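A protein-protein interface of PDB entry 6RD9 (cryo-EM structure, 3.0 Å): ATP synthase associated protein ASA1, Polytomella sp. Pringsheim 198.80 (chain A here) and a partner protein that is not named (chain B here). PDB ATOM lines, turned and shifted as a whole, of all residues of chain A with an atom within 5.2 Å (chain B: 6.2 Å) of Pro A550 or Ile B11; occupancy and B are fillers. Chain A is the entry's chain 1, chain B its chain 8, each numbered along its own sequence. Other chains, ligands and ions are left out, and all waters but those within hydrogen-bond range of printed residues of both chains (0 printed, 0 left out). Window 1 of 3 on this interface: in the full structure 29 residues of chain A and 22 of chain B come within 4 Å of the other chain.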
ATOM      1  N   VAL A 545      31.029  -2.743  -5.577  1.00  0.00           N
ATOM      2  CA  VAL A 545      30.384  -1.631  -6.260  1.00  0.00           C
ATOM      3  C   VAL A 545      29.195  -2.122  -7.062  1.00  0.00           C
ATOM      4  O   VAL A 545      28.106  -1.557  -7.001  1.00  0.00           O
ATOM      5  CB  VAL A 545      31.391  -0.923  -7.166  1.00  0.00           C
ATOM      6  CG1 VAL A 545      30.709   0.065  -7.986  1.00  0.00           C
ATOM      7  CG2 VAL A 545      32.419  -0.285  -6.377  1.00  0.00           C
ATOM      8  N   ALA A 546      29.378  -3.193  -7.814  1.00  0.00           N
ATOM      9  CA  ALA A 546      28.297  -3.725  -8.616  1.00  0.00           C
ATOM     10  C   ALA A 546      27.267  -4.440  -7.785  1.00  0.00           C
ATOM     11  O   ALA A 546      26.191  -4.748  -8.291  1.00  0.00           O
ATOM     12  CB  ALA A 546      28.849  -4.671  -9.661  1.00  0.00           C
ATOM     13  N   HIS A 547      27.586  -4.765  -6.543  1.00  0.00           N
ATOM     14  CA  HIS A 547      26.578  -5.274  -5.639  1.00  0.00           C
ATOM     15  C   HIS A 547      25.756  -4.139  -5.083  1.00  0.00           C
ATOM     16  O   HIS A 547      24.531  -4.159  -5.162  1.00  0.00           O
ATOM     17  CB  HIS A 547      27.227  -6.042  -4.504  1.00  0.00           C
ATOM     18  CG  HIS A 547      26.241  -6.614  -3.550  1.00  0.00           C
ATOM     19  ND1 HIS A 547      26.034  -6.102  -2.295  1.00  0.00           N
ATOM     20  CD2 HIS A 547      25.378  -7.642  -3.684  1.00  0.00           C
ATOM     21  CE1 HIS A 547      25.092  -6.794  -1.689  1.00  0.00           C
ATOM     22  NE2 HIS A 547      24.673  -7.733  -2.514  1.00  0.00           N
ATOM     23  N   MET A 548      26.430  -3.133  -4.545  1.00  0.00           N
ATOM     24  CA  MET A 548      25.769  -2.001  -3.930  1.00  0.00           C
ATOM     25  C   MET A 548      24.995  -1.191  -4.944  1.00  0.00           C
ATOM     26  O   MET A 548      23.850  -0.819  -4.703  1.00  0.00           O
ATOM     27  CB  MET A 548      26.798  -1.121  -3.256  1.00  0.00           C
ATOM     28  CG  MET A 548      27.156  -1.510  -1.911  1.00  0.00           C
ATOM     29  SD  MET A 548      27.912  -0.098  -1.187  1.00  0.00           S
ATOM     30  CE  MET A 548      29.544  -0.355  -1.742  1.00  0.00           C
ATOM     31  N   ASP A 549      25.590  -0.907  -6.088  1.00  0.00           N
ATOM     32  CA  ASP A 549      24.955  -0.082  -7.103  1.00  0.00           C
ATOM     33  C   ASP A 549      24.898  -0.866  -8.398  1.00  0.00           C
ATOM     34  O   ASP A 549      25.774  -0.723  -9.251  1.00  0.00           O
ATOM     35  CB  ASP A 549      25.702   1.226  -7.290  1.00  0.00           C
ATOM     36  CG  ASP A 549      24.774   2.366  -7.534  1.00  0.00           C
ATOM     37  OD1 ASP A 549      23.579   2.102  -7.698  1.00  0.00           O
ATOM     38  OD2 ASP A 549      25.214   3.526  -7.499  1.00  0.00           O
ATOM     39  N   PRO A 550      23.893  -1.718  -8.573  1.00  0.00           N
ATOM     40  CA  PRO A 550      23.866  -2.550  -9.766  1.00  0.00           C
ATOM     41  C   PRO A 550      23.392  -1.825 -10.996  1.00  0.00           C
ATOM     42  O   PRO A 550      23.782  -2.206 -12.098  1.00  0.00           O
ATOM     43  CB  PRO A 550      22.913  -3.670  -9.368  1.00  0.00           C
ATOM     44  CG  PRO A 550      22.068  -3.098  -8.405  1.00  0.00           C
ATOM     45  CD  PRO A 550      22.835  -2.107  -7.640  1.00  0.00           C
ATOM     46  N   LEU A 551      22.554  -0.816 -10.859  1.00  0.00           N
ATOM     47  CA  LEU A 551      22.068  -0.088 -12.009  1.00  0.00           C
ATOM     48  C   LEU A 551      22.979   1.040 -12.412  1.00  0.00           C
ATOM     49  O   LEU A 551      22.766   1.622 -13.461  1.00  0.00           O
ATOM     50  CB  LEU A 551      20.687   0.491 -11.741  1.00  0.00           C
ATOM     51  CG  LEU A 551      19.506  -0.414 -11.487  1.00  0.00           C
ATOM     52  CD1 LEU A 551      18.307   0.424 -11.311  1.00  0.00           C
ATOM     53  CD2 LEU A 551      19.315  -1.290 -12.647  1.00  0.00           C
ATOM     54  N   LEU A 552      23.943   1.408 -11.590  1.00  0.00           N
ATOM     55  CA  LEU A 552      24.957   2.340 -12.053  1.00  0.00           C
ATOM     56  C   LEU A 552      25.956   1.627 -12.923  1.00  0.00           C
ATOM     57  O   LEU A 552      26.363   2.141 -13.959  1.00  0.00           O
ATOM     58  CB  LEU A 552      25.669   2.986 -10.881  1.00  0.00           C
ATOM     59  CG  LEU A 552      26.769   3.956 -11.250  1.00  0.00           C
ATOM     60  CD1 LEU A 552      26.208   5.119 -11.961  1.00  0.00           C
ATOM     61  CD2 LEU A 552      27.487   4.399 -10.061  1.00  0.00           C
ATOM     62  N   ILE A 553      26.342   0.426 -12.519  1.00  0.00           N
ATOM     63  CA  ILE A 553      27.202  -0.432 -13.311  1.00  0.00           C
ATOM     64  C   ILE A 553      26.510  -0.855 -14.590  1.00  0.00           C
ATOM     65  O   ILE A 553      27.147  -0.951 -15.630  1.00  0.00           O
ATOM     66  CB  ILE A 553      27.611  -1.615 -12.427  1.00  0.00           C
ATOM     67  CG1 ILE A 553      28.468  -1.120 -11.278  1.00  0.00           C
ATOM     68  CG2 ILE A 553      28.292  -2.673 -13.171  1.00  0.00           C
ATOM     69  CD1 ILE A 553      29.635  -0.332 -11.683  1.00  0.00           C
ATOM     70  N   LYS A 554      25.200  -1.054 -14.555  1.00  0.00           N
ATOM     71  CA  LYS A 554      24.439  -1.417 -15.742  1.00  0.00           C
ATOM     72  C   LYS A 554      24.420  -0.297 -16.762  1.00  0.00           C
ATOM     73  O   LYS A 554      24.504  -0.550 -17.960  1.00  0.00           O
ATOM     74  CB  LYS A 554      23.019  -1.773 -15.346  1.00  0.00           C
ATOM     75  CG  LYS A 554      22.164  -2.261 -16.459  1.00  0.00           C
ATOM     76  CD  LYS A 554      20.742  -1.987 -16.177  1.00  0.00           C
ATOM     77  CE  LYS A 554      19.886  -2.455 -17.278  1.00  0.00           C
ATOM     78  NZ  LYS A 554      18.514  -1.979 -17.065  1.00  0.00           N
ATOM     79  N   HIS A 590      18.306   6.552 -10.736  1.00  0.00           N
ATOM     80  CA  HIS A 590      17.645   5.435 -10.118  1.00  0.00           C
ATOM     81  C   HIS A 590      17.794   5.430  -8.621  1.00  0.00           C
ATOM     82  O   HIS A 590      17.319   4.502  -7.978  1.00  0.00           O
ATOM     83  CB  HIS A 590      18.229   4.156 -10.666  1.00  0.00           C
ATOM     84  CG  HIS A 590      19.705   4.062 -10.475  1.00  0.00           C
ATOM     85  ND1 HIS A 590      20.268   3.387  -9.424  1.00  0.00           N
ATOM     86  CD2 HIS A 590      20.731   4.590 -11.172  1.00  0.00           C
ATOM     87  CE1 HIS A 590      21.576   3.495  -9.487  1.00  0.00           C
ATOM     88  NE2 HIS A 590      21.882   4.216 -10.542  1.00  0.00           N
ATOM     89  N   LEU A 593      14.393   6.320  -7.495  1.00  0.00           N
ATOM     90  CA  LEU A 593      13.342   5.389  -7.881  1.00  0.00           C
ATOM     91  C   LEU A 593      12.698   4.629  -6.723  1.00  0.00           C
ATOM     92  O   LEU A 593      11.479   4.407  -6.797  1.00  0.00           O
ATOM     93  CB  LEU A 593      13.882   4.414  -8.924  1.00  0.00           C
ATOM     94  CG  LEU A 593      12.898   3.420  -9.504  1.00  0.00           C
ATOM     95  CD1 LEU A 593      11.809   4.177 -10.163  1.00  0.00           C
ATOM     96  CD2 LEU A 593      13.571   2.540 -10.462  1.00  0.00           C
ATOM     97  N   PRO A 594      13.389   4.201  -5.656  1.00  0.00           N
ATOM     98  CA  PRO A 594      12.647   3.619  -4.539  1.00  0.00           C
ATOM     99  C   PRO A 594      11.742   4.584  -3.824  1.00  0.00           C
ATOM    100  O   PRO A 594      10.822   4.144  -3.141  1.00  0.00           O
ATOM    101  CB  PRO A 594      13.753   3.138  -3.615  1.00  0.00           C
ATOM    102  CG  PRO A 594      14.823   2.889  -4.453  1.00  0.00           C
ATOM    103  CD  PRO A 594      14.818   3.943  -5.441  1.00  0.00           C
ATOM    104  N   ARG A 597       8.622   5.262  -6.533  1.00  0.00           N
ATOM    105  CA  ARG A 597       7.738   4.118  -6.634  1.00  0.00           C
ATOM    106  C   ARG A 597       6.933   3.941  -5.373  1.00  0.00           C
ATOM    107  O   ARG A 597       5.876   3.320  -5.409  1.00  0.00           O
ATOM    108  CB  ARG A 597       8.526   2.850  -6.874  1.00  0.00           C
ATOM    109  CG  ARG A 597       8.883   2.643  -8.267  1.00  0.00           C
ATOM    110  CD  ARG A 597       9.638   1.372  -8.413  1.00  0.00           C
ATOM    111  NE  ARG A 597       8.811   0.192  -8.291  1.00  0.00           N
ATOM    112  CZ  ARG A 597       8.084  -0.298  -9.282  1.00  0.00           C
ATOM    113  NH1 ARG A 597       8.072   0.302 -10.456  1.00  0.00           N
ATOM    114  NH2 ARG A 597       7.370  -1.387  -9.104  1.00  0.00           N
ATOM    115  N   TYR B   7      10.866  -1.904  -2.282  1.00  0.00           N
ATOM    116  CA  TYR B   7      11.090  -0.804  -3.192  1.00  0.00           C
ATOM    117  C   TYR B   7      12.554  -0.602  -3.489  1.00  0.00           C
ATOM    118  O   TYR B   7      12.884  -0.062  -4.542  1.00  0.00           O
ATOM    119  CB  TYR B   7      10.504   0.480  -2.622  1.00  0.00           C
ATOM    120  CG  TYR B   7       9.021   0.432  -2.479  1.00  0.00           C
ATOM    121  CD1 TYR B   7       8.207   0.546  -3.582  1.00  0.00           C
ATOM    122  CD2 TYR B   7       8.433   0.280  -1.247  1.00  0.00           C
ATOM    123  CE1 TYR B   7       6.855   0.505  -3.464  1.00  0.00           C
ATOM    124  CE2 TYR B   7       7.081   0.232  -1.117  1.00  0.00           C
ATOM    125  CZ  TYR B   7       6.297   0.346  -2.227  1.00  0.00           C
ATOM    126  OH  TYR B   7       4.936   0.301  -2.097  1.00  0.00           O
ATOM    127  N   LEU B   8      13.429  -1.023  -2.598  1.00  0.00           N
ATOM    128  CA  LEU B   8      14.858  -0.948  -2.817  1.00  0.00           C
ATOM    129  C   LEU B   8      15.424  -2.197  -3.454  1.00  0.00           C
ATOM    130  O   LEU B   8      16.640  -2.312  -3.552  1.00  0.00           O
ATOM    131  CB  LEU B   8      15.585  -0.738  -1.503  1.00  0.00           C
ATOM    132  CG  LEU B   8      15.380   0.434  -0.582  1.00  0.00           C
ATOM    133  CD1 LEU B   8      16.133   0.052   0.585  1.00  0.00           C
ATOM    134  CD2 LEU B   8      16.007   1.623  -1.130  1.00  0.00           C
ATOM    135  N   LYS B   9      14.597  -3.151  -3.846  1.00  0.00           N
ATOM    136  CA  LYS B   9      15.114  -4.416  -4.340  1.00  0.00           C
ATOM    137  C   LYS B   9      15.665  -4.254  -5.740  1.00  0.00           C
ATOM    138  O   LYS B   9      14.980  -3.744  -6.627  1.00  0.00           O
ATOM    139  CB  LYS B   9      14.028  -5.477  -4.341  1.00  0.00           C
ATOM    140  CG  LYS B   9      14.554  -6.859  -4.569  1.00  0.00           C
ATOM    141  CD  LYS B   9      13.445  -7.830  -4.806  1.00  0.00           C
ATOM    142  CE  LYS B   9      12.914  -7.723  -6.215  1.00  0.00           C
ATOM    143  NZ  LYS B   9      13.746  -8.472  -7.182  1.00  0.00           N
ATOM    144  N   ASP B  10      16.920  -4.682  -5.910  1.00  0.00           N
ATOM    145  CA  ASP B  10      17.674  -4.646  -7.161  1.00  0.00           C
ATOM    146  C   ASP B  10      17.867  -3.233  -7.674  1.00  0.00           C
ATOM    147  O   ASP B  10      18.020  -3.018  -8.869  1.00  0.00           O
ATOM    148  CB  ASP B  10      17.039  -5.522  -8.233  1.00  0.00           C
ATOM    149  CG  ASP B  10      16.973  -6.967  -7.828  1.00  0.00           C
ATOM    150  OD1 ASP B  10      17.812  -7.393  -7.016  1.00  0.00           O
ATOM    151  OD2 ASP B  10      16.091  -7.686  -8.328  1.00  0.00           O
ATOM    152  N   ILE B  11      17.866  -2.265  -6.773  1.00  0.00           N
ATOM    153  CA  ILE B  11      18.043  -0.869  -7.115  1.00  0.00           C
ATOM    154  C   ILE B  11      19.187  -0.350  -6.275  1.00  0.00           C
ATOM    155  O   ILE B  11      20.177   0.165  -6.799  1.00  0.00           O
ATOM    156  CB  ILE B  11      16.767  -0.058  -6.873  1.00  0.00           C
ATOM    157  CG1 ILE B  11      15.701  -0.434  -7.880  1.00  0.00           C
ATOM    158  CG2 ILE B  11      17.053   1.364  -7.038  1.00  0.00           C
ATOM    159  CD1 ILE B  11      14.383   0.151  -7.605  1.00  0.00           C
ATOM    160  N   LEU B  12      19.063  -0.493  -4.964  1.00  0.00           N
ATOM    161  CA  LEU B  12      20.049  -0.011  -4.017  1.00  0.00           C
ATOM    162  C   LEU B  12      20.304  -1.101  -3.008  1.00  0.00           C
ATOM    163  O   LEU B  12      19.382  -1.521  -2.315  1.00  0.00           O
ATOM    164  CB  LEU B  12      19.562   1.230  -3.290  1.00  0.00           C
ATOM    165  CG  LEU B  12      19.502   2.555  -4.009  1.00  0.00           C
ATOM    166  CD1 LEU B  12      18.598   3.391  -3.214  1.00  0.00           C
ATOM    167  CD2 LEU B  12      20.850   3.156  -4.045  1.00  0.00           C
ATOM    168  N   ARG B  13      21.540  -1.547  -2.910  1.00  0.00           N
ATOM    169  CA  ARG B  13      21.910  -2.505  -1.893  1.00  0.00           C
ATOM    170  C   ARG B  13      22.954  -1.880  -0.991  1.00  0.00           C
ATOM    171  O   ARG B  13      23.617  -0.923  -1.365  1.00  0.00           O
ATOM    172  CB  ARG B  13      22.427  -3.771  -2.511  1.00  0.00           C
ATOM    173  CG  ARG B  13      21.566  -4.274  -3.605  1.00  0.00           C
ATOM    174  CD  ARG B  13      21.845  -5.689  -3.864  1.00  0.00           C
ATOM    175  NE  ARG B  13      20.998  -6.200  -4.915  1.00  0.00           N
ATOM    176  CZ  ARG B  13      21.392  -6.386  -6.158  1.00  0.00           C
ATOM    177  NH1 ARG B  13      20.558  -6.864  -7.051  1.00  0.00           N
ATOM    178  NH2 ARG B  13      22.621  -6.108  -6.501  1.00  0.00           N
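The backbone carbonyl oxygen (O) of His A547 sits at hydrogen-bond distance from the guanidinium group (NH2) of Arg B13, 3.0 Å away. N of Arg B13 lies within hydrogen-bond range of O of Met A548 (3.0 Å).
The side-chain amino group of Lys B9 lies within salt-bridge range of the side-chain carboxylate of Asp B10 (2.7 Å). OD1 of Asp B10 lies within salt-bridge range of NH1 of Arg B13, 2.8 Å away.
O of Met A548 touches C of Leu B12, 3.9 Å away. Ile B11 touches Pro A550. CG of Pro A550 touches NH2 of Arg B13 (3.6 Å). Leu A551 touches Asp B10 (CG to O, 3.98 Å). Ile B11 touches His A590 (CG2 to O, 3.3 Å). CD2 of Leu A593 touches CD1 of Ile B11 (3.8 Å). CB of Pro A594 touches O of Tyr B7, 3.4 Å away. Pro A594 touches Leu B8. Pro A594 touches Ile B11. Tyr B7 touches Arg A597.
Of chain B, only Ile B11 and Arg B13 come within 4 Å of Pro A550. Of the printed residues of chain A, Ile B11 touches Pro A550, His A590, Leu A593 and Pro A594. Printed residues of chain B within 4 Å of Met A548: Leu B12 (3.9 Å) and Arg B13 (3.0 Å). Printed residues of chain A within 4 Å of Leu B8: Pro A594. Printed residues of chain A within 4 Å of Leu B12: Met A548 (3.9 Å). Of the printed residues of chain B, His A547 touches Arg B13 (3.0 Å). Printed residues of chain A within 4 Å of Arg B13: His A547, Met A548 and Pro A550.
Hydrophobic or aromatic side chains of chain B within 4 Å of the printed part of chain A: Tyr B7, Leu B8 and Ile B11. Hydrophobic or aromatic side chains of chain A that line the printed part of chain B: His A547, Met A548, Pro A550, Leu A551, Leu A593 and Pro A594. Among the printed residues, 12 pairs touch across the chains. Among the printed residues, no Asp or Glu carboxylate lies within 4 Å of a Lys or Arg side-chain nitrogen of the other chain.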
